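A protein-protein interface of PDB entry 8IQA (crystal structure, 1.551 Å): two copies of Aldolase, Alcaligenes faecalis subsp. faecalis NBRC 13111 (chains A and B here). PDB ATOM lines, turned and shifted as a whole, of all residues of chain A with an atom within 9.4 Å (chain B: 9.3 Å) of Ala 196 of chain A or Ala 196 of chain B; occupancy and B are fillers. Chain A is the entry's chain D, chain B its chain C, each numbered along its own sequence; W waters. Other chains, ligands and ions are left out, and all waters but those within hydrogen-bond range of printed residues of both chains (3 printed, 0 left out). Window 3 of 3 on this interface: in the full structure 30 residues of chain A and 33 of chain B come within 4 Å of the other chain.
NE2 of Gln 191 of chain B sits at hydrogen-bond distance from OE1 of Gln 195 of chain B, at 3.0 Å.
Among the printed residues, merely in contact across the chains: Leu 190 of chain A with Val 109 of chain B (3.7 Å), Arg 193 of chain A with Trp 106 of chain B (3.5 Å), Arg 193 of chain A with Val 109 of chain B (3.9 Å), Ala 194 of chain A with Val 109 of chain B (3.6 Å), Ala 196 of chain A with Ala 196 of chain B (3.6 Å), Ala 197 of chain A with Val 192 of chain B (3.7 Å), Ala 197 of chain A with Ala 196 of chain B (3.7 Å), Phe 198 of chain A with Ala 113 of chain B (3.3 Å) and Phe 198 of chain A with Gln 195 of chain B (3.4 Å).
Ala 196 of chain A touches one residue of chain B.
Of the printed residues of chain A, Gln 195 of chain B touches Phe 198.
Printed residues of chain B within 4 Å of Phe 198 of chain A: Ala 113 (3.3 Å) and Gln 195 (3.4 Å).
Pro 200 of chain A touches none of the printed residues of chain B.
Arg 189 of chain B touches none of the printed residues of chain A.
The nearest residue of chain A that does not touch Ala 196 of chain B is Arg 193 of chain A (5.6 Å).
The nearest printed residue of chain B that does not touch Phe 198 of chain A is Val 109 of chain B (4.1 Å).
Hydrophobic or aromatic side chains of chain B within 4 Å of the printed part of chain A: Trp 106, Val 109, Ala 113, Val 192 and Ala 196.
Of the 16 printed residues of chain A, 6 touch a printed residue of chain B.
Hydrophobic or aromatic side chains of chain A within 4 Å of the printed part of chain B: Leu 190, Ala 194, Ala 197 and Phe 198.
Among the printed residues, 9 pairs touch across the chains.
Arg 193 of chain A touches Val 109 of chain B, but with the chains exchanged Val 109 of chain A does not touch Arg 193 of chain B (14.9 Å).
Ala 194 of chain A touches Val 109 of chain B, but with the chains exchanged Val 109 of chain A does not touch Ala 194 of chain B (17.2 Å).
Ala 196 of chain A touches its own counterpart, Ala 196 of chain B.
Ala 197 of chain A touches Val 192 of chain B, but with the chains exchanged Val 192 of chain A does not touch Ala 197 of chain B (10.3 Å).
16 positions are printed for both chains.
Of the 9 pairs that touch across the chains among the printed residues, 1 has its exchanged pair printed and touching as well.
Water W3 bridges O of Ala 197 of chain A (2.7 Å) and NE2 of Gln 195 of chain B (3.0 Å).
Water W1 lies within hydrogen-bond range of O of Gln 195 of chain B (2.8 Å) and O of Ala 197 of chain A (3.3 Å).
Water W2 bridges O of Ala 196 of chain A (2.9 Å) and O of Ala 196 of chain B (3.1 Å).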
ATOM      1  N   TRP A 106      -3.768  10.200  13.474  1.00  0.00           N
ATOM      2  CA  TRP A 106      -3.428   8.798  13.711  1.00  0.00           C
ATOM      3  C   TRP A 106      -1.952   8.535  13.835  1.00  0.00           C
ATOM      4  O   TRP A 106      -1.535   7.803  14.742  1.00  0.00           O
ATOM      5  CB  TRP A 106      -4.068   7.949  12.623  1.00  0.00           C
ATOM      6  CG  TRP A 106      -5.570   8.007  12.683  1.00  0.00           C
ATOM      7  CD1 TRP A 106      -6.397   8.781  11.919  1.00  0.00           C
ATOM      8  CD2 TRP A 106      -6.416   7.279  13.586  1.00  0.00           C
ATOM      9  NE1 TRP A 106      -7.708   8.565  12.281  1.00  0.00           N
ATOM     10  CE2 TRP A 106      -7.748   7.609  13.268  1.00  0.00           C
ATOM     11  CE3 TRP A 106      -6.180   6.344  14.603  1.00  0.00           C
ATOM     12  CZ2 TRP A 106      -8.832   7.028  13.919  1.00  0.00           C
ATOM     13  CZ3 TRP A 106      -7.267   5.734  15.221  1.00  0.00           C
ATOM     14  CH2 TRP A 106      -8.568   6.107  14.907  1.00  0.00           C
ATOM     15  N   VAL A 109      -0.959   9.183  17.236  1.00  0.00           N
ATOM     16  CA  VAL A 109      -1.275   8.172  18.254  1.00  0.00           C
ATOM     17  C   VAL A 109      -0.055   7.256  18.381  1.00  0.00           C
ATOM     18  O   VAL A 109       0.373   6.962  19.508  1.00  0.00           O
ATOM     19  CB  VAL A 109      -2.506   7.337  17.846  1.00  0.00           C
ATOM     20  CG1 VAL A 109      -2.667   6.118  18.783  1.00  0.00           C
ATOM     21  CG2 VAL A 109      -3.773   8.199  17.816  1.00  0.00           C
ATOM     22  N   ALA A 188      -0.935   4.353   9.942  1.00  0.00           N
ATOM     23  CA  ALA A 188      -1.067   4.498  11.395  1.00  0.00           C
ATOM     24  C   ALA A 188      -2.543   4.252  11.818  1.00  0.00           C
ATOM     25  O   ALA A 188      -2.806   3.502  12.759  1.00  0.00           O
ATOM     26  CB  ALA A 188      -0.627   5.899  11.807  1.00  0.00           C
ATOM     27  N   ARG A 189      -3.499   4.800  11.065  1.00  0.00           N
ATOM     28  CA  ARG A 189      -4.943   4.592  11.367  1.00  0.00           C
ATOM     29  C   ARG A 189      -5.304   3.124  11.331  1.00  0.00           C
ATOM     30  O   ARG A 189      -5.986   2.622  12.245  1.00  0.00           O
ATOM     31  CB  ARG A 189      -5.803   5.330  10.328  1.00  0.00           C
ATOM     32  CG  ARG A 189      -7.298   5.239  10.617  1.00  0.00           C
ATOM     33  CD  ARG A 189      -8.077   6.127   9.648  1.00  0.00           C
ATOM     34  NE  ARG A 189      -7.996   5.598   8.290  1.00  0.00           N
ATOM     35  CZ  ARG A 189      -8.532   6.187   7.227  1.00  0.00           C
ATOM     36  NH1 ARG A 189      -9.137   7.362   7.346  1.00  0.00           N
ATOM     37  NH2 ARG A 189      -8.413   5.635   6.026  1.00  0.00           N
ATOM     38  N   LEU A 190      -4.840   2.419  10.286  1.00  0.00           N
ATOM     39  CA  LEU A 190      -5.113   0.996  10.129  1.00  0.00           C
ATOM     40  C   LEU A 190      -4.517   0.214  11.310  1.00  0.00           C
ATOM     41  O   LEU A 190      -5.212  -0.608  11.914  1.00  0.00           O
ATOM     42  CB  LEU A 190      -4.491   0.547   8.808  1.00  0.00           C
ATOM     43  CG  LEU A 190      -4.548  -0.929   8.521  1.00  0.00           C
ATOM     44  CD1 LEU A 190      -6.009  -1.398   8.436  1.00  0.00           C
ATOM     45  CD2 LEU A 190      -3.894  -1.232   7.199  1.00  0.00           C
ATOM     46  N   GLN A 191      -3.263   0.501  11.666  1.00  0.00           N
ATOM     47  CA  GLN A 191      -2.604  -0.210  12.762  1.00  0.00           C
ATOM     48  C   GLN A 191      -3.272   0.049  14.114  1.00  0.00           C
ATOM     49  O   GLN A 191      -3.479  -0.905  14.866  1.00  0.00           O
ATOM     50  CB  GLN A 191      -1.127   0.168  12.837  1.00  0.00           C
ATOM     51  CG  GLN A 191      -0.390  -0.517  14.026  1.00  0.00           C
ATOM     52  CD  GLN A 191       1.113  -0.336  13.933  1.00  0.00           C
ATOM     53  OE1 GLN A 191       1.649  -0.023  12.861  1.00  0.00           O
ATOM     54  NE2 GLN A 191       1.820  -0.537  15.048  1.00  0.00           N
ATOM     55  N   VAL A 192      -3.612   1.298  14.418  1.00  0.00           N
ATOM     56  CA  VAL A 192      -4.230   1.626  15.693  1.00  0.00           C
ATOM     57  C   VAL A 192      -5.623   0.945  15.799  1.00  0.00           C
ATOM     58  O   VAL A 192      -5.931   0.327  16.817  1.00  0.00           O
ATOM     59  CB  VAL A 192      -4.316   3.164  15.885  1.00  0.00           C
ATOM     60  CG1 VAL A 192      -5.122   3.509  17.134  1.00  0.00           C
ATOM     61  CG2 VAL A 192      -2.913   3.768  15.995  1.00  0.00           C
ATOM     62  N   ARG A 193      -6.432   1.031  14.730  1.00  0.00           N
ATOM     63  CA  ARG A 193      -7.760   0.415  14.733  1.00  0.00           C
ATOM     64  C   ARG A 193      -7.633  -1.102  14.869  1.00  0.00           C
ATOM     65  O   ARG A 193      -8.351  -1.687  15.664  1.00  0.00           O
ATOM     66  CB  ARG A 193      -8.507   0.731  13.438  1.00  0.00           C
ATOM     67  CG  ARG A 193      -9.075   2.135  13.446  1.00  0.00           C
ATOM     68  CD  ARG A 193      -9.616   2.503  12.083  1.00  0.00           C
ATOM     69  NE  ARG A 193     -10.388   3.738  12.139  1.00  0.00           N
ATOM     70  CZ  ARG A 193     -10.925   4.335  11.083  1.00  0.00           C
ATOM     71  NH1 ARG A 193     -10.739   3.838   9.861  1.00  0.00           N
ATOM     72  NH2 ARG A 193     -11.683   5.420  11.241  1.00  0.00           N
ATOM     73  N   ALA A 194      -6.672  -1.711  14.167  1.00  0.00           N
ATOM     74  CA  ALA A 194      -6.493  -3.166  14.232  1.00  0.00           C
ATOM     75  C   ALA A 194      -5.985  -3.627  15.590  1.00  0.00           C
ATOM     76  O   ALA A 194      -6.509  -4.597  16.112  1.00  0.00           O
ATOM     77  CB  ALA A 194      -5.541  -3.647  13.124  1.00  0.00           C
ATOM     78  N   GLN A 195      -5.014  -2.909  16.204  1.00  0.00           N
ATOM     79  CA  GLN A 195      -4.514  -3.321  17.510  1.00  0.00           C
ATOM     80  C   GLN A 195      -5.539  -3.116  18.599  1.00  0.00           C
ATOM     81  O   GLN A 195      -5.620  -3.939  19.515  1.00  0.00           O
ATOM     82  CB  GLN A 195      -3.184  -2.591  17.863  1.00  0.00           C
ATOM     83  CG  GLN A 195      -2.095  -3.047  16.911  1.00  0.00           C
ATOM     84  CD  GLN A 195      -0.706  -2.838  17.453  1.00  0.00           C
ATOM     85  OE1 GLN A 195       0.163  -2.360  16.742  1.00  0.00           O
ATOM     86  NE2 GLN A 195      -0.458  -3.222  18.706  1.00  0.00           N
ATOM     87  N   ALA A 196      -6.366  -2.065  18.501  1.00  0.00           N
ATOM     88  CA  ALA A 196      -7.421  -1.850  19.515  1.00  0.00           C
ATOM     89  C   ALA A 196      -8.392  -3.028  19.555  1.00  0.00           C
ATOM     90  O   ALA A 196      -8.802  -3.469  20.634  1.00  0.00           O
ATOM     91  CB  ALA A 196      -8.190  -0.571  19.205  1.00  0.00           C
ATOM     92  N   ALA A 197      -8.711  -3.573  18.372  1.00  0.00           N
ATOM     93  CA  ALA A 197      -9.679  -4.678  18.309  1.00  0.00           C
ATOM     94  C   ALA A 197      -9.047  -6.048  18.510  1.00  0.00           C
ATOM     95  O   ALA A 197      -9.701  -6.922  19.094  1.00  0.00           O
ATOM     96  CB  ALA A 197     -10.382  -4.670  16.938  1.00  0.00           C
ATOM     97  N   PHE A 198      -7.821  -6.256  17.991  1.00  0.00           N
ATOM     98  CA  PHE A 198      -7.242  -7.596  17.912  1.00  0.00           C
ATOM     99  C   PHE A 198      -5.848  -7.797  18.516  1.00  0.00           C
ATOM    100  O   PHE A 198      -5.332  -8.914  18.452  1.00  0.00           O
ATOM    101  CB  PHE A 198      -7.210  -8.044  16.415  1.00  0.00           C
ATOM    102  CG  PHE A 198      -8.544  -7.898  15.700  1.00  0.00           C
ATOM    103  CD1 PHE A 198      -9.624  -8.679  16.054  1.00  0.00           C
ATOM    104  CD2 PHE A 198      -8.727  -6.927  14.732  1.00  0.00           C
ATOM    105  CE1 PHE A 198     -10.863  -8.497  15.448  1.00  0.00           C
ATOM    106  CE2 PHE A 198      -9.948  -6.804  14.069  1.00  0.00           C
ATOM    107  CZ  PHE A 198     -11.009  -7.581  14.439  1.00  0.00           C
ATOM    108  N   GLY A 199      -5.236  -6.749  19.058  1.00  0.00           N
ATOM    109  CA  GLY A 199      -3.891  -6.866  19.614  1.00  0.00           C
ATOM    110  C   GLY A 199      -2.791  -6.715  18.584  1.00  0.00           C
ATOM    111  O   GLY A 199      -3.046  -6.351  17.436  1.00  0.00           O
ATOM    112  N   PRO A 200      -1.522  -6.984  18.978  1.00  0.00           N
ATOM    113  CA  PRO A 200      -0.401  -6.829  18.040  1.00  0.00           C
ATOM    114  C   PRO A 200      -0.581  -7.603  16.729  1.00  0.00           C
ATOM    115  O   PRO A 200      -1.133  -8.709  16.704  1.00  0.00           O
ATOM    116  CB  PRO A 200       0.803  -7.350  18.836  1.00  0.00           C
ATOM    117  CG  PRO A 200       0.423  -7.122  20.285  1.00  0.00           C
ATOM    118  CD  PRO A 200      -1.062  -7.416  20.316  1.00  0.00           C
ATOM    119  N   LEU A 201      -0.122  -7.004  15.643  1.00  0.00           N
ATOM    120  CA  LEU A 201      -0.282  -7.559  14.310  1.00  0.00           C
ATOM    121  C   LEU A 201       0.869  -8.442  13.892  1.00  0.00           C
ATOM    122  O   LEU A 201       1.994  -8.222  14.335  1.00  0.00           O
ATOM    123  CB  LEU A 201      -0.298  -6.364  13.343  1.00  0.00           C
ATOM    124  CG  LEU A 201      -1.469  -5.391  13.527  1.00  0.00           C
ATOM    125  CD1 LEU A 201      -1.288  -4.162  12.622  1.00  0.00           C
ATOM    126  CD2 LEU A 201      -2.801  -6.120  13.273  1.00  0.00           C
ATOM    127  N   TRP B 106     -12.417  -0.059   6.937  1.00  0.00           N
ATOM    128  CA  TRP B 106     -12.762  -1.054   7.972  1.00  0.00           C
ATOM    129  C   TRP B 106     -12.565  -2.494   7.516  1.00  0.00           C
ATOM    130  O   TRP B 106     -12.039  -3.314   8.267  1.00  0.00           O
ATOM    131  CB  TRP B 106     -14.175  -0.794   8.451  1.00  0.00           C
ATOM    132  CG  TRP B 106     -14.299   0.550   9.131  1.00  0.00           C
ATOM    133  CD1 TRP B 106     -14.785   1.703   8.587  1.00  0.00           C
ATOM    134  CD2 TRP B 106     -13.889   0.867  10.456  1.00  0.00           C
ATOM    135  NE1 TRP B 106     -14.749   2.716   9.518  1.00  0.00           N
ATOM    136  CE2 TRP B 106     -14.226   2.221  10.689  1.00  0.00           C
ATOM    137  CE3 TRP B 106     -13.303   0.129  11.496  1.00  0.00           C
ATOM    138  CZ2 TRP B 106     -13.993   2.850  11.905  1.00  0.00           C
ATOM    139  CZ3 TRP B 106     -13.121   0.746  12.720  1.00  0.00           C
ATOM    140  CH2 TRP B 106     -13.421   2.101  12.901  1.00  0.00           C
ATOM    141  N   VAL B 109      -9.066  -3.396   7.967  1.00  0.00           N
ATOM    142  CA  VAL B 109      -8.677  -3.732   9.336  1.00  0.00           C
ATOM    143  C   VAL B 109      -8.783  -5.225   9.530  1.00  0.00           C
ATOM    144  O   VAL B 109      -7.829  -5.858   9.996  1.00  0.00           O
ATOM    145  CB  VAL B 109      -9.516  -2.991  10.392  1.00  0.00           C
ATOM    146  CG1 VAL B 109      -9.158  -3.499  11.794  1.00  0.00           C
ATOM    147  CG2 VAL B 109      -9.309  -1.487  10.290  1.00  0.00           C
ATOM    148  N   ALA B 113      -5.565  -7.688  10.249  1.00  0.00           N
ATOM    149  CA  ALA B 113      -5.516  -8.509  11.443  1.00  0.00           C
ATOM    150  C   ALA B 113      -5.748  -9.996  11.169  1.00  0.00           C
ATOM    151  O   ALA B 113      -5.804 -10.781  12.126  1.00  0.00           O
ATOM    152  CB  ALA B 113      -6.534  -8.007  12.449  1.00  0.00           C
ATOM    153  N   ALA B 188     -17.743  -4.921   8.589  1.00  0.00           N
ATOM    154  CA  ALA B 188     -16.393  -4.906   9.141  1.00  0.00           C
ATOM    155  C   ALA B 188     -16.283  -3.777  10.207  1.00  0.00           C
ATOM    156  O   ALA B 188     -15.752  -4.002  11.292  1.00  0.00           O
ATOM    157  CB  ALA B 188     -15.375  -4.663   8.026  1.00  0.00           C
ATOM    158  N   ARG B 189     -16.840  -2.585   9.918  1.00  0.00           N
ATOM    159  CA  ARG B 189     -16.812  -1.476  10.889  1.00  0.00           C
ATOM    160  C   ARG B 189     -17.498  -1.878  12.186  1.00  0.00           C
ATOM    161  O   ARG B 189     -16.971  -1.622  13.277  1.00  0.00           O
ATOM    162  CB  ARG B 189     -17.548  -0.274  10.273  1.00  0.00           C
ATOM    163  CG  ARG B 189     -17.537   0.971  11.175  1.00  0.00           C
ATOM    164  CD  ARG B 189     -18.170   2.151  10.457  1.00  0.00           C
ATOM    165  NE  ARG B 189     -19.600   1.933  10.287  1.00  0.00           N
ATOM    166  CZ  ARG B 189     -20.428   2.749   9.637  1.00  0.00           C
ATOM    167  NH1 ARG B 189     -19.960   3.816   9.011  1.00  0.00           N
ATOM    168  NH2 ARG B 189     -21.723   2.457   9.546  1.00  0.00           N
ATOM    169  N   LEU B 190     -18.714  -2.511  12.072  1.00  0.00           N
ATOM    170  CA  LEU B 190     -19.457  -2.923  13.240  1.00  0.00           C
ATOM    171  C   LEU B 190     -18.631  -3.940  14.057  1.00  0.00           C
ATOM    172  O   LEU B 190     -18.518  -3.805  15.279  1.00  0.00           O
ATOM    173  CB  LEU B 190     -20.772  -3.585  12.745  1.00  0.00           C
ATOM    174  CG  LEU B 190     -21.635  -4.191  13.812  1.00  0.00           C
ATOM    175  CD1 LEU B 190     -22.032  -3.125  14.894  1.00  0.00           C
ATOM    176  CD2 LEU B 190     -22.904  -4.742  13.153  1.00  0.00           C
ATOM    177  N   GLN B 191     -18.037  -4.922  13.386  1.00  0.00           N
ATOM    178  CA  GLN B 191     -17.242  -5.943  14.079  1.00  0.00           C
ATOM    179  C   GLN B 191     -16.003  -5.391  14.749  1.00  0.00           C
ATOM    180  O   GLN B 191     -15.743  -5.746  15.885  1.00  0.00           O
ATOM    181  CB  GLN B 191     -16.855  -7.069  13.109  1.00  0.00           C
ATOM    182  CG  GLN B 191     -15.985  -8.167  13.768  1.00  0.00           C
ATOM    183  CD  GLN B 191     -15.854  -9.376  12.865  1.00  0.00           C
ATOM    184  OE1 GLN B 191     -16.640  -9.559  11.925  1.00  0.00           O
ATOM    185  NE2 GLN B 191     -14.846 -10.221  13.121  1.00  0.00           N
ATOM    186  N   VAL B 192     -15.257  -4.524  14.067  1.00  0.00           N
ATOM    187  CA  VAL B 192     -14.048  -3.955  14.655  1.00  0.00           C
ATOM    188  C   VAL B 192     -14.399  -3.082  15.884  1.00  0.00           C
ATOM    189  O   VAL B 192     -13.759  -3.191  16.944  1.00  0.00           O
ATOM    190  CB  VAL B 192     -13.263  -3.171  13.583  1.00  0.00           C
ATOM    191  CG1 VAL B 192     -12.107  -2.389  14.208  1.00  0.00           C
ATOM    192  CG2 VAL B 192     -12.749  -4.135  12.505  1.00  0.00           C
ATOM    193  N   ARG B 193     -15.402  -2.218  15.754  1.00  0.00           N
ATOM    194  CA  ARG B 193     -15.818  -1.361  16.878  1.00  0.00           C
ATOM    195  C   ARG B 193     -16.305  -2.229  18.052  1.00  0.00           C
ATOM    196  O   ARG B 193     -15.953  -1.960  19.202  1.00  0.00           O
ATOM    197  CB  ARG B 193     -16.938  -0.426  16.441  1.00  0.00           C
ATOM    198  CG  ARG B 193     -16.460   0.709  15.561  1.00  0.00           C
ATOM    199  CD  ARG B 193     -17.638   1.495  15.029  1.00  0.00           C
ATOM    200  NE  ARG B 193     -17.204   2.754  14.417  1.00  0.00           N
ATOM    201  CZ  ARG B 193     -18.013   3.597  13.783  1.00  0.00           C
ATOM    202  NH1 ARG B 193     -19.302   3.312  13.640  1.00  0.00           N
ATOM    203  NH2 ARG B 193     -17.550   4.757  13.338  1.00  0.00           N
ATOM    204  N   ALA B 194     -17.083  -3.290  17.755  1.00  0.00           N
ATOM    205  CA  ALA B 194     -17.579  -4.164  18.814  1.00  0.00           C
ATOM    206  C   ALA B 194     -16.472  -4.940  19.496  1.00  0.00           C
ATOM    207  O   ALA B 194     -16.460  -5.017  20.727  1.00  0.00           O
ATOM    208  CB  ALA B 194     -18.667  -5.097  18.296  1.00  0.00           C
ATOM    209  N   GLN B 195     -15.524  -5.499  18.732  1.00  0.00           N
ATOM    210  CA  GLN B 195     -14.453  -6.284  19.346  1.00  0.00           C
ATOM    211  C   GLN B 195     -13.497  -5.397  20.137  1.00  0.00           C
ATOM    212  O   GLN B 195     -13.018  -5.820  21.203  1.00  0.00           O
ATOM    213  CB  GLN B 195     -13.705  -7.119  18.288  1.00  0.00           C
ATOM    214  CG  GLN B 195     -14.630  -8.199  17.736  1.00  0.00           C
ATOM    215  CD  GLN B 195     -13.875  -9.355  17.123  1.00  0.00           C
ATOM    216  OE1 GLN B 195     -14.197  -9.808  16.027  1.00  0.00           O
ATOM    217  NE2 GLN B 195     -12.869  -9.861  17.831  1.00  0.00           N
ATOM    218  N   ALA B 196     -13.269  -4.151  19.686  1.00  0.00           N
ATOM    219  CA  ALA B 196     -12.358  -3.256  20.427  1.00  0.00           C
ATOM    220  C   ALA B 196     -12.921  -2.989  21.849  1.00  0.00           C
ATOM    221  O   ALA B 196     -12.170  -2.942  22.809  1.00  0.00           O
ATOM    222  CB  ALA B 196     -12.219  -1.929  19.686  1.00  0.00           C
ATOM    223  N   ALA B 197     -14.247  -2.874  21.963  1.00  0.00           N
ATOM    224  CA  ALA B 197     -14.847  -2.586  23.267  1.00  0.00           C
ATOM    225  C   ALA B 197     -15.154  -3.837  24.077  1.00  0.00           C
ATOM    226  O   ALA B 197     -15.057  -3.815  25.309  1.00  0.00           O
ATOM    227  CB  ALA B 197     -16.142  -1.789  23.070  1.00  0.00           C
ATOM    228  N   PHE B 198     -15.569  -4.915  23.400  1.00  0.00           N
ATOM    229  CA  PHE B 198     -16.137  -6.082  24.114  1.00  0.00           C
ATOM    230  C   PHE B 198     -15.528  -7.448  23.819  1.00  0.00           C
ATOM    231  O   PHE B 198     -16.004  -8.425  24.375  1.00  0.00           O
ATOM    232  CB  PHE B 198     -17.663  -6.146  23.800  1.00  0.00           C
ATOM    233  CG  PHE B 198     -18.395  -4.843  24.060  1.00  0.00           C
ATOM    234  CD1 PHE B 198     -18.507  -4.332  25.349  1.00  0.00           C
ATOM    235  CD2 PHE B 198     -18.909  -4.097  23.008  1.00  0.00           C
ATOM    236  CE1 PHE B 198     -19.146  -3.106  25.583  1.00  0.00           C
ATOM    237  CE2 PHE B 198     -19.591  -2.900  23.248  1.00  0.00           C
ATOM    238  CZ  PHE B 198     -19.673  -2.390  24.529  1.00  0.00           C
ATOM    239  N   GLY B 199     -14.512  -7.515  22.954  1.00  0.00           N
ATOM    240  CA  GLY B 199     -13.909  -8.796  22.588  1.00  0.00           C
ATOM    241  C   GLY B 199     -14.698  -9.574  21.542  1.00  0.00           C
ATOM    242  O   GLY B 199     -15.625  -9.046  20.902  1.00  0.00           O
ATOM    243  N   PRO B 200     -14.310 -10.832  21.319  1.00  0.00           N
ATOM    244  CA  PRO B 200     -14.972 -11.640  20.274  1.00  0.00           C
ATOM    245  C   PRO B 200     -16.499 -11.731  20.400  1.00  0.00           C
ATOM    246  O   PRO B 200     -17.047 -11.778  21.491  1.00  0.00           O
ATOM    247  CB  PRO B 200     -14.320 -13.026  20.436  1.00  0.00           C
ATOM    248  CG  PRO B 200     -12.964 -12.725  20.984  1.00  0.00           C
ATOM    249  CD  PRO B 200     -13.191 -11.575  21.950  1.00  0.00           C
ATOM    250  N   LEU B 201     -17.168 -11.737  19.269  1.00  0.00           N
ATOM    251  CA  LEU B 201     -18.618 -11.729  19.183  1.00  0.00           C
ATOM    252  C   LEU B 201     -19.235 -13.123  19.117  1.00  0.00           C
ATOM    253  O   LEU B 201     -18.604 -14.060  18.663  1.00  0.00           O
ATOM    254  CB  LEU B 201     -19.015 -11.005  17.887  1.00  0.00           C
ATOM    255  CG  LEU B 201     -18.570  -9.543  17.783  1.00  0.00           C
ATOM    256  CD1 LEU B 201     -18.873  -9.013  16.407  1.00  0.00           C
ATOM    257  CD2 LEU B 201     -19.250  -8.721  18.846  1.00  0.00           C
HETATM  258  O   HOH W   1     -10.426  -6.251  22.245  1.00  0.00           O
HETATM  259  O   HOH W   2      -9.218  -2.279  23.263  1.00  0.00           O
HETATM  260  O   HOH W   3     -11.008  -9.032  20.023  1.00  0.00           O
